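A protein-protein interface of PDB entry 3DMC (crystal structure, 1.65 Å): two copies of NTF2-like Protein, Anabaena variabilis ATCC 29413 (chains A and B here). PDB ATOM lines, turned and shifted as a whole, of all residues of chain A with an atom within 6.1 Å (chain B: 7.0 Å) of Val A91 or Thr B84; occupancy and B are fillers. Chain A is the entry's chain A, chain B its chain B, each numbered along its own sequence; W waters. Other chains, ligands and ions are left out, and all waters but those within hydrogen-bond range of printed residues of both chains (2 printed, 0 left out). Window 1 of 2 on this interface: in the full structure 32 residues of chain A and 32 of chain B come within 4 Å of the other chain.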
ATOM      1  N   GLY A   1      24.241   6.233 -12.693  1.00  0.00           N
ATOM      2  CA  GLY A   1      25.438   6.077 -11.788  1.00  0.00           C
ATOM      3  C   GLY A   1      25.838   7.342 -11.073  1.00  0.00           C
ATOM      4  O   GLY A   1      25.503   8.461 -11.483  1.00  0.00           O
ATOM      5  N   ARG A  82      16.286  18.021 -10.970  1.00  0.00           N
ATOM      6  CA  ARG A  82      17.024  16.763 -10.877  1.00  0.00           C
ATOM      7  C   ARG A  82      17.295  16.215 -12.257  1.00  0.00           C
ATOM      8  O   ARG A  82      16.400  16.162 -13.087  1.00  0.00           O
ATOM      9  CB  ARG A  82      16.242  15.743 -10.028  1.00  0.00           C
ATOM     10  CG  ARG A  82      15.993  16.203  -8.590  1.00  0.00           C
ATOM     11  CD  ARG A  82      15.206  15.228  -7.733  1.00  0.00           C
ATOM     12  NE  ARG A  82      15.373  15.539  -6.317  1.00  0.00           N
ATOM     13  CZ  ARG A  82      14.754  16.540  -5.688  1.00  0.00           C
ATOM     14  NH1 ARG A  82      13.904  17.337  -6.338  1.00  0.00           N
ATOM     15  NH2 ARG A  82      14.991  16.759  -4.403  1.00  0.00           N
ATOM     16  N   VAL A  83      18.552  15.849 -12.470  1.00  0.00           N
ATOM     17  CA  VAL A  83      18.971  15.207 -13.711  1.00  0.00           C
ATOM     18  C   VAL A  83      19.732  13.944 -13.355  1.00  0.00           C
ATOM     19  O   VAL A  83      20.813  13.982 -12.751  1.00  0.00           O
ATOM     20  CB  VAL A  83      19.879  16.147 -14.506  1.00  0.00           C
ATOM     21  CG1 VAL A  83      20.379  15.470 -15.764  1.00  0.00           C
ATOM     22  CG2 VAL A  83      19.103  17.429 -14.865  1.00  0.00           C
ATOM     23  N   THR A  84      19.167  12.821 -13.762  1.00  0.00           N
ATOM     24  CA  THR A  84      19.767  11.520 -13.456  1.00  0.00           C
ATOM     25  C   THR A  84      20.078  10.785 -14.733  1.00  0.00           C
ATOM     26  O   THR A  84      19.478  11.043 -15.759  1.00  0.00           O
ATOM     27  CB  THR A  84      18.799  10.660 -12.593  1.00  0.00           C
ATOM     28  OG1 THR A  84      17.549  10.553 -13.264  1.00  0.00           O
ATOM     29  CG2 THR A  84      18.587  11.252 -11.155  1.00  0.00           C
ATOM     30  N   SER A  85      21.067   9.887 -14.678  1.00  0.00           N
ATOM     31  CA  SER A  85      21.433   9.141 -15.883  1.00  0.00           C
ATOM     32  C   SER A  85      21.986   7.760 -15.584  1.00  0.00           C
ATOM     33  O   SER A  85      22.269   7.381 -14.444  1.00  0.00           O
ATOM     34  CB  SER A  85      22.428   9.936 -16.755  1.00  0.00           C
ATOM     35  OG  SER A  85      23.712  10.094 -16.178  1.00  0.00           O
ATOM     36  N   ASN A  86      22.124   7.055 -16.677  1.00  0.00           N
ATOM     37  CA  ASN A  86      22.862   5.765 -16.722  1.00  0.00           C
ATOM     38  C   ASN A  86      23.668   5.729 -18.024  1.00  0.00           C
ATOM     39  O   ASN A  86      23.990   6.782 -18.575  1.00  0.00           O
ATOM     40  CB  ASN A  86      21.943   4.554 -16.510  1.00  0.00           C
ATOM     41  CG  ASN A  86      20.883   4.371 -17.595  1.00  0.00           C
ATOM     42  OD1 ASN A  86      21.061   4.770 -18.726  1.00  0.00           O
ATOM     43  ND2 ASN A  86      19.763   3.687 -17.237  1.00  0.00           N
ATOM     44  N   THR A  89      20.455   6.570 -20.793  1.00  0.00           N
ATOM     45  CA  THR A  89      19.209   7.275 -20.521  1.00  0.00           C
ATOM     46  C   THR A  89      19.495   8.431 -19.580  1.00  0.00           C
ATOM     47  O   THR A  89      20.294   8.307 -18.643  1.00  0.00           O
ATOM     48  CB  THR A  89      18.172   6.335 -19.847  1.00  0.00           C
ATOM     49  OG1 THR A  89      17.904   5.197 -20.675  1.00  0.00           O
ATOM     50  CG2 THR A  89      16.854   7.030 -19.577  1.00  0.00           C
ATOM     51  N   VAL A  90      18.814   9.540 -19.844  1.00  0.00           N
ATOM     52  CA  VAL A  90      18.853  10.708 -18.944  1.00  0.00           C
ATOM     53  C   VAL A  90      17.439  11.158 -18.668  1.00  0.00           C
ATOM     54  O   VAL A  90      16.586  11.221 -19.583  1.00  0.00           O
ATOM     55  CB  VAL A  90      19.635  11.890 -19.540  1.00  0.00           C
ATOM     56  CG1 VAL A  90      19.800  12.935 -18.485  1.00  0.00           C
ATOM     57  CG2 VAL A  90      21.027  11.412 -20.066  1.00  0.00           C
ATOM     58  N   VAL A  91      17.178  11.447 -17.401  1.00  0.00           N
ATOM     59  CA  VAL A  91      15.853  11.959 -17.001  1.00  0.00           C
ATOM     60  C   VAL A  91      16.047  13.322 -16.384  1.00  0.00           C
ATOM     61  O   VAL A  91      16.955  13.543 -15.573  1.00  0.00           O
ATOM     62  CB  VAL A  91      15.140  11.065 -15.933  1.00  0.00           C
ATOM     63  CG1 VAL A  91      13.753  11.630 -15.524  1.00  0.00           C
ATOM     64  CG2 VAL A  91      14.982   9.615 -16.398  1.00  0.00           C
ATOM     65  N   PHE A  92      15.188  14.214 -16.841  1.00  0.00           N
ATOM     66  CA  PHE A  92      15.096  15.599 -16.405  1.00  0.00           C
ATOM     67  C   PHE A  92      13.781  15.765 -15.656  1.00  0.00           C
ATOM     68  O   PHE A  92      12.724  15.607 -16.229  1.00  0.00           O
ATOM     69  CB  PHE A  92      15.114  16.513 -17.639  1.00  0.00           C
ATOM     70  CG  PHE A  92      16.388  16.446 -18.417  1.00  0.00           C
ATOM     71  CD1 PHE A  92      16.556  15.467 -19.435  1.00  0.00           C
ATOM     72  CD2 PHE A  92      17.421  17.342 -18.174  1.00  0.00           C
ATOM     73  CE1 PHE A  92      17.725  15.397 -20.140  1.00  0.00           C
ATOM     74  CE2 PHE A  92      18.593  17.266 -18.900  1.00  0.00           C
ATOM     75  CZ  PHE A  92      18.745  16.296 -19.869  1.00  0.00           C
ATOM     76  N   GLU A  93      13.883  16.114 -14.378  1.00  0.00           N
ATOM     77  CA  GLU A  93      12.733  16.415 -13.557  1.00  0.00           C
ATOM     78  C   GLU A  93      12.709  17.930 -13.416  1.00  0.00           C
ATOM     79  O   GLU A  93      13.644  18.547 -12.847  1.00  0.00           O
ATOM     80  CB  GLU A  93      12.819  15.774 -12.175  1.00  0.00           C
ATOM     81  CG  GLU A  93      12.746  14.263 -12.148  1.00  0.00           C
ATOM     82  CD  GLU A  93      12.903  13.722 -10.742  1.00  0.00           C
ATOM     83  OE1 GLU A  93      12.078  14.136  -9.871  1.00  0.00           O
ATOM     84  OE2 GLU A  93      13.834  12.906 -10.526  1.00  0.00           O
ATOM     85  N   ALA A 110       8.529  14.979 -15.802  1.00  0.00           N
ATOM     86  CA  ALA A 110       9.754  14.259 -16.022  1.00  0.00           C
ATOM     87  C   ALA A 110       9.787  13.836 -17.480  1.00  0.00           C
ATOM     88  O   ALA A 110       8.869  13.234 -17.984  1.00  0.00           O
ATOM     89  CB  ALA A 110       9.863  13.045 -15.116  1.00  0.00           C
ATOM     90  N   VAL A 111      10.846  14.223 -18.163  1.00  0.00           N
ATOM     91  CA  VAL A 111      11.101  13.692 -19.497  1.00  0.00           C
ATOM     92  C   VAL A 111      12.404  12.916 -19.492  1.00  0.00           C
ATOM     93  O   VAL A 111      13.433  13.351 -18.966  1.00  0.00           O
ATOM     94  CB  VAL A 111      11.106  14.758 -20.617  1.00  0.00           C
ATOM     95  CG1 VAL A 111       9.772  15.551 -20.621  1.00  0.00           C
ATOM     96  CG2 VAL A 111      12.336  15.672 -20.528  1.00  0.00           C
ATOM     97  N   SER A 112      12.311  11.757 -20.120  1.00  0.00           N
ATOM     98  CA  SER A 112      13.367  10.777 -20.186  1.00  0.00           C
ATOM     99  C   SER A 112      13.798  10.630 -21.648  1.00  0.00           C
ATOM    100  O   SER A 112      12.957  10.479 -22.520  1.00  0.00           O
ATOM    101  CB  SER A 112      12.834   9.442 -19.638  1.00  0.00           C
ATOM    102  OG  SER A 112      13.831   8.449 -19.620  1.00  0.00           O
ATOM    103  N   PHE A 113      15.095  10.779 -21.890  1.00  0.00           N
ATOM    104  CA  PHE A 113      15.661  10.550 -23.241  1.00  0.00           C
ATOM    105  C   PHE A 113      16.562   9.307 -23.228  1.00  0.00           C
ATOM    106  O   PHE A 113      17.325   9.089 -22.266  1.00  0.00           O
ATOM    107  CB  PHE A 113      16.603  11.717 -23.684  1.00  0.00           C
ATOM    108  CG  PHE A 113      15.976  13.094 -23.727  1.00  0.00           C
ATOM    109  CD1 PHE A 113      14.638  13.281 -23.897  1.00  0.00           C
ATOM    110  CD2 PHE A 113      16.793  14.231 -23.706  1.00  0.00           C
ATOM    111  CE1 PHE A 113      14.079  14.554 -23.962  1.00  0.00           C
ATOM    112  CE2 PHE A 113      16.247  15.483 -23.778  1.00  0.00           C
ATOM    113  CZ  PHE A 113      14.878  15.652 -23.926  1.00  0.00           C
ATOM    114  N   GLY B   1      24.857   9.854 -13.790  1.00  0.00           N
ATOM    115  CA  GLY B   1      26.232   9.602 -14.346  1.00  0.00           C
ATOM    116  C   GLY B   1      26.325   8.261 -15.031  1.00  0.00           C
ATOM    117  O   GLY B   1      25.568   7.324 -14.722  1.00  0.00           O
ATOM    118  N   LEU B  11      22.625   4.278  -5.453  1.00  0.00           N
ATOM    119  CA  LEU B  11      21.993   3.164  -6.220  1.00  0.00           C
ATOM    120  C   LEU B  11      21.601   2.002  -5.325  1.00  0.00           C
ATOM    121  O   LEU B  11      20.486   1.486  -5.388  1.00  0.00           O
ATOM    122  CB  LEU B  11      22.890   2.630  -7.354  1.00  0.00           C
ATOM    123  CG  LEU B  11      22.673   3.126  -8.780  1.00  0.00           C
ATOM    124  CD1 LEU B  11      23.597   2.352  -9.735  1.00  0.00           C
ATOM    125  CD2 LEU B  11      21.204   2.980  -9.174  1.00  0.00           C
ATOM    126  N   ARG B  82      13.869   1.298 -16.902  1.00  0.00           N
ATOM    127  CA  ARG B  82      15.017   2.201 -16.842  1.00  0.00           C
ATOM    128  C   ARG B  82      15.241   2.680 -15.435  1.00  0.00           C
ATOM    129  O   ARG B  82      14.290   3.065 -14.773  1.00  0.00           O
ATOM    130  CB  ARG B  82      14.773   3.411 -17.731  1.00  0.00           C
ATOM    131  CG  ARG B  82      14.593   3.041 -19.206  1.00  0.00           C
ATOM    132  CD  ARG B  82      14.308   4.236 -20.096  1.00  0.00           C
ATOM    133  NE  ARG B  82      14.563   3.905 -21.496  1.00  0.00           N
ATOM    134  CZ  ARG B  82      13.736   3.202 -22.271  1.00  0.00           C
ATOM    135  NH1 ARG B  82      12.571   2.743 -21.795  1.00  0.00           N
ATOM    136  NH2 ARG B  82      14.085   2.942 -23.525  1.00  0.00           N
ATOM    137  N   VAL B  83      16.490   2.631 -15.007  1.00  0.00           N
ATOM    138  CA  VAL B  83      16.884   3.148 -13.655  1.00  0.00           C
ATOM    139  C   VAL B  83      18.063   4.083 -13.895  1.00  0.00           C
ATOM    140  O   VAL B  83      19.135   3.667 -14.388  1.00  0.00           O
ATOM    141  CB  VAL B  83      17.353   2.028 -12.714  1.00  0.00           C
ATOM    142  CG1 VAL B  83      17.779   2.591 -11.357  1.00  0.00           C
ATOM    143  CG2 VAL B  83      16.213   1.027 -12.517  1.00  0.00           C
ATOM    144  N   THR B  84      17.867   5.346 -13.537  1.00  0.00           N
ATOM    145  CA  THR B  84      18.905   6.359 -13.716  1.00  0.00           C
ATOM    146  C   THR B  84      19.249   6.974 -12.386  1.00  0.00           C
ATOM    147  O   THR B  84      18.463   6.934 -11.451  1.00  0.00           O
ATOM    148  CB  THR B  84      18.437   7.490 -14.693  1.00  0.00           C
ATOM    149  OG1 THR B  84      17.167   7.991 -14.275  1.00  0.00           O
ATOM    150  CG2 THR B  84      18.331   6.966 -16.205  1.00  0.00           C
ATOM    151  N   SER B  85      20.460   7.513 -12.276  1.00  0.00           N
ATOM    152  CA  SER B  85      20.850   8.126 -11.001  1.00  0.00           C
ATOM    153  C   SER B  85      21.886   9.245 -11.140  1.00  0.00           C
ATOM    154  O   SER B  85      22.429   9.506 -12.185  1.00  0.00           O
ATOM    155  CB  SER B  85      21.345   7.049 -10.040  1.00  0.00           C
ATOM    156  OG  SER B  85      22.626   6.545 -10.399  1.00  0.00           O
ATOM    157  N   ASN B  86      22.107   9.879 -10.023  1.00  0.00           N
ATOM    158  CA  ASN B  86      23.214  10.825  -9.845  1.00  0.00           C
ATOM    159  C   ASN B  86      23.756  10.641  -8.420  1.00  0.00           C
ATOM    160  O   ASN B  86      23.635   9.556  -7.840  1.00  0.00           O
ATOM    161  CB  ASN B  86      22.806  12.258 -10.168  1.00  0.00           C
ATOM    162  CG  ASN B  86      21.706  12.802  -9.299  1.00  0.00           C
ATOM    163  OD1 ASN B  86      21.557  12.434  -8.133  1.00  0.00           O
ATOM    164  ND2 ASN B  86      20.959  13.804  -9.846  1.00  0.00           N
ATOM    165  N   THR B  89      20.055  11.077  -6.204  1.00  0.00           N
ATOM    166  CA  THR B  89      18.729  10.750  -6.700  1.00  0.00           C
ATOM    167  C   THR B  89      18.767   9.546  -7.642  1.00  0.00           C
ATOM    168  O   THR B  89      19.741   9.330  -8.388  1.00  0.00           O
ATOM    169  CB  THR B  89      18.127  11.981  -7.448  1.00  0.00           C
ATOM    170  OG1 THR B  89      18.087  13.112  -6.574  1.00  0.00           O
ATOM    171  CG2 THR B  89      16.727  11.733  -7.951  1.00  0.00           C
ATOM    172  N   VAL B  90      17.710   8.741  -7.535  1.00  0.00           N
ATOM    173  CA  VAL B  90      17.494   7.615  -8.462  1.00  0.00           C
ATOM    174  C   VAL B  90      16.070   7.641  -8.981  1.00  0.00           C
ATOM    175  O   VAL B  90      15.116   7.839  -8.215  1.00  0.00           O
ATOM    176  CB  VAL B  90      17.762   6.247  -7.753  1.00  0.00           C
ATOM    177  CG1 VAL B  90      17.755   5.152  -8.757  1.00  0.00           C
ATOM    178  CG2 VAL B  90      19.121   6.285  -7.043  1.00  0.00           C
ATOM    179  N   VAL B  91      15.923   7.432 -10.288  1.00  0.00           N
ATOM    180  CA  VAL B  91      14.592   7.326 -10.887  1.00  0.00           C
ATOM    181  C   VAL B  91      14.412   5.929 -11.462  1.00  0.00           C
ATOM    182  O   VAL B  91      15.293   5.396 -12.136  1.00  0.00           O
ATOM    183  CB  VAL B  91      14.357   8.389 -12.004  1.00  0.00           C
ATOM    184  CG1 VAL B  91      12.976   8.267 -12.582  1.00  0.00           C
ATOM    185  CG2 VAL B  91      14.565   9.823 -11.467  1.00  0.00           C
ATOM    186  N   PHE B  92      13.250   5.377 -11.128  1.00  0.00           N
ATOM    187  CA  PHE B  92      12.772   4.105 -11.635  1.00  0.00           C
ATOM    188  C   PHE B  92      11.614   4.365 -12.584  1.00  0.00           C
ATOM    189  O   PHE B  92      10.606   4.887 -12.165  1.00  0.00           O
ATOM    190  CB  PHE B  92      12.304   3.250 -10.472  1.00  0.00           C
ATOM    191  CG  PHE B  92      13.386   2.931  -9.473  1.00  0.00           C
ATOM    192  CD1 PHE B  92      13.702   3.823  -8.441  1.00  0.00           C
ATOM    193  CD2 PHE B  92      14.089   1.738  -9.550  1.00  0.00           C
ATOM    194  CE1 PHE B  92      14.694   3.527  -7.518  1.00  0.00           C
ATOM    195  CE2 PHE B  92      15.094   1.455  -8.622  1.00  0.00           C
ATOM    196  CZ  PHE B  92      15.391   2.366  -7.613  1.00  0.00           C
ATOM    197  N   GLU B  93      11.775   3.946 -13.843  1.00  0.00           N
ATOM    198  CA  GLU B  93      10.717   4.017 -14.820  1.00  0.00           C
ATOM    199  C   GLU B  93      10.219   2.588 -14.992  1.00  0.00           C
ATOM    200  O   GLU B  93      10.983   1.689 -15.387  1.00  0.00           O
ATOM    201  CB  GLU B  93      11.219   4.553 -16.169  1.00  0.00           C
ATOM    202  CG  GLU B  93      11.582   6.019 -16.189  1.00  0.00           C
ATOM    203  CD  GLU B  93      12.148   6.423 -17.524  1.00  0.00           C
ATOM    204  OE1 GLU B  93      11.423   6.327 -18.539  1.00  0.00           O
ATOM    205  OE2 GLU B  93      13.321   6.821 -17.547  1.00  0.00           O
ATOM    206  N   ALA B 110       6.921   6.831 -13.204  1.00  0.00           N
ATOM    207  CA  ALA B 110       8.299   7.133 -12.781  1.00  0.00           C
ATOM    208  C   ALA B 110       8.238   7.554 -11.317  1.00  0.00           C
ATOM    209  O   ALA B 110       7.463   8.426 -10.954  1.00  0.00           O
ATOM    210  CB  ALA B 110       8.966   8.240 -13.625  1.00  0.00           C
ATOM    211  N   TYR B 126       5.408  10.309 -10.817  1.00  0.00           N
ATOM    212  CA  TYR B 126       4.919  10.869 -12.087  1.00  0.00           C
ATOM    213  C   TYR B 126       4.153   9.787 -12.877  1.00  0.00           C
ATOM    214  O   TYR B 126       4.549   8.618 -12.873  1.00  0.00           O
ATOM    215  CB  TYR B 126       6.101  11.348 -12.933  1.00  0.00           C
ATOM    216  CG  TYR B 126       7.063  12.336 -12.311  1.00  0.00           C
ATOM    217  CD1 TYR B 126       8.088  11.908 -11.460  1.00  0.00           C
ATOM    218  CD2 TYR B 126       6.966  13.716 -12.576  1.00  0.00           C
ATOM    219  CE1 TYR B 126       9.026  12.834 -10.914  1.00  0.00           C
ATOM    220  CE2 TYR B 126       7.868  14.649 -11.995  1.00  0.00           C
ATOM    221  CZ  TYR B 126       8.886  14.187 -11.150  1.00  0.00           C
ATOM    222  OH  TYR B 126       9.748  15.113 -10.621  1.00  0.00           O
HETATM  223  O   HOH W   1      20.715  16.951 -10.683  1.00  0.00           O
HETATM  224  O   HOH W   2      18.392   0.805 -16.240  1.00  0.00           O
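Water W2 lies within hydrogen-bond range of N of Val B83 (2.9 Å) and ND2 of Asn A86 (3.3 Å).
Water W1 bridges the backbone NH of Val A83 (3.0 Å) and the side-chain amide nitrogen of Asn B86 (3.3 Å).
Of the 14 printed residues of chain B, 10 touch a printed residue of chain A.
Printed residues of chain B that touch a printed residue of chain A: Gly B1, Arg B82, Val B83, Thr B84, Ser B85, Asn B86, Thr B89, Val B91, Glu B93 and Tyr B126.
Hydrophobic or aromatic side chains of chain B that line the printed part of chain A: Val B91 and Tyr B126.
Among the printed residues, no Asp or Glu carboxylate lies within 4 Å of a Lys or Arg side-chain nitrogen of the other chain.
The backbone NH of Gly A1 lies within hydrogen-bond range of the backbone carbonyl oxygen of Ser A85 (2.9 Å).
The backbone carbonyl oxygen (O) of Thr A84 sits at hydrogen-bond distance from the backbone NH (N) of Val A91.
The side-chain amide oxygen (OD1) of Asn A86 sits at hydrogen-bond distance from the backbone NH (N) of Thr A89.
N of Gly B1 lies within hydrogen-bond range of O of Ser B85.
The backbone carbonyl oxygen (O) of Thr B84 is in hydrogen-bond range of the backbone NH (N) of Val B91 (2.8 Å).
The backbone carbonyl oxygen (O) of Ala B110 is in hydrogen-bond range of the backbone NH (N) of Tyr B126, at 2.8 Å.
Gly A1 touches its own counterpart, Gly B1.
Gly A1 touches Ser B85, and with the chains exchanged Ser A85 touches Gly B1.
Gly A1 touches Asn B86, and with the chains exchanged Asn A86 touches Gly B1.
Thr A84 touches Ser B85, and with the chains exchanged Ser A85 touches Thr B84.
O of Gly B1 is in hydrogen-bond range of N of Gly A1, 2.7 Å away.
The backbone NH (N) of Gly A1 lies within hydrogen-bond range of the side-chain hydroxyl (OG) of Ser B85, 2.8 Å away.
The side-chain amide nitrogen of Asn B86 sits at hydrogen-bond distance from the backbone carbonyl oxygen of Val A83 (2.9 Å).
OG1 of Thr B84 is in hydrogen-bond range of OG1 of Thr A84 (2.8 Å).
N of Gly B1 sits at hydrogen-bond distance from OG of Ser A85, 2.7 Å away.
The backbone NH of Ser B85 lies within hydrogen-bond range of the backbone carbonyl oxygen of Ser A85, at 2.8 Å.
O of Val B83 sits at hydrogen-bond distance from ND2 of Asn A86 (2.9 Å).
The side-chain carboxylate of Glu A93 lies within hydrogen-bond range of the side-chain hydroxyl of Tyr B126 (2.6 Å).
The side-chain carboxylate of Glu B93 is in hydrogen-bond range of the side-chain hydroxyl of Ser A112, 2.7 Å away.
Val A91 touches just these residues of chain B: Thr B84 (3.5 Å) and Glu B93 (3.4 Å).
Thr B84 touches just these residues of chain A: Thr A84, Ser A85, Asn A86, Thr A89 and Val A91.
Of the printed residues of chain B, Asn A86 touches Gly B1 (3.7 Å), Val B83 (2.9 Å) and Thr B84 (3.7 Å).
Of the printed residues of chain B, Arg A82 touches Thr B89.
Printed residues of chain A within 4 Å of Ser B85: Gly A1 (2.8 Å), Thr A84 (3.6 Å) and Ser A85 (2.8 Å).
Of the printed residues of chain B, Gly A1 touches Gly B1, Ser B85 and Asn B86.
Printed residues of chain B within 4 Å of Ser A85: Gly B1 (2.7 Å), Thr B84 (3.6 Å) and Ser B85 (2.8 Å).
Val A111 touches none of the printed residues of chain B.
Val B90 touches none of the printed residues of chain A.
The nearest residue of chain A that does not touch Thr B84 is Val A90 (4.5 Å).
Among the printed residues, pairs that only touch across the chains: Gly A1 with Asn B86 (3.7 Å), Arg A82 with Thr B89 (3.6 Å), Thr A84 with Ser B85 (3.6 Å), Thr A84 with Asn B86 (3.7 Å), Thr A84 with Thr B89 (3.6 Å), Thr A84 with Val B91 (3.6 Å), Ser A85 with Thr B84 (3.6 Å), Asn A86 with Gly B1 (3.7 Å), Asn A86 with Thr B84 (3.7 Å), Thr A89 with Arg B82 (3.7 Å), Thr A89 with Thr B84 (3.4 Å), Val A91 with Thr B84 (3.5 Å), Val A91 with Glu B93 (3.4 Å), Glu A93 with Val B91 (3.3 Å) and Ala A110 with Tyr B126 (3.8 Å).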
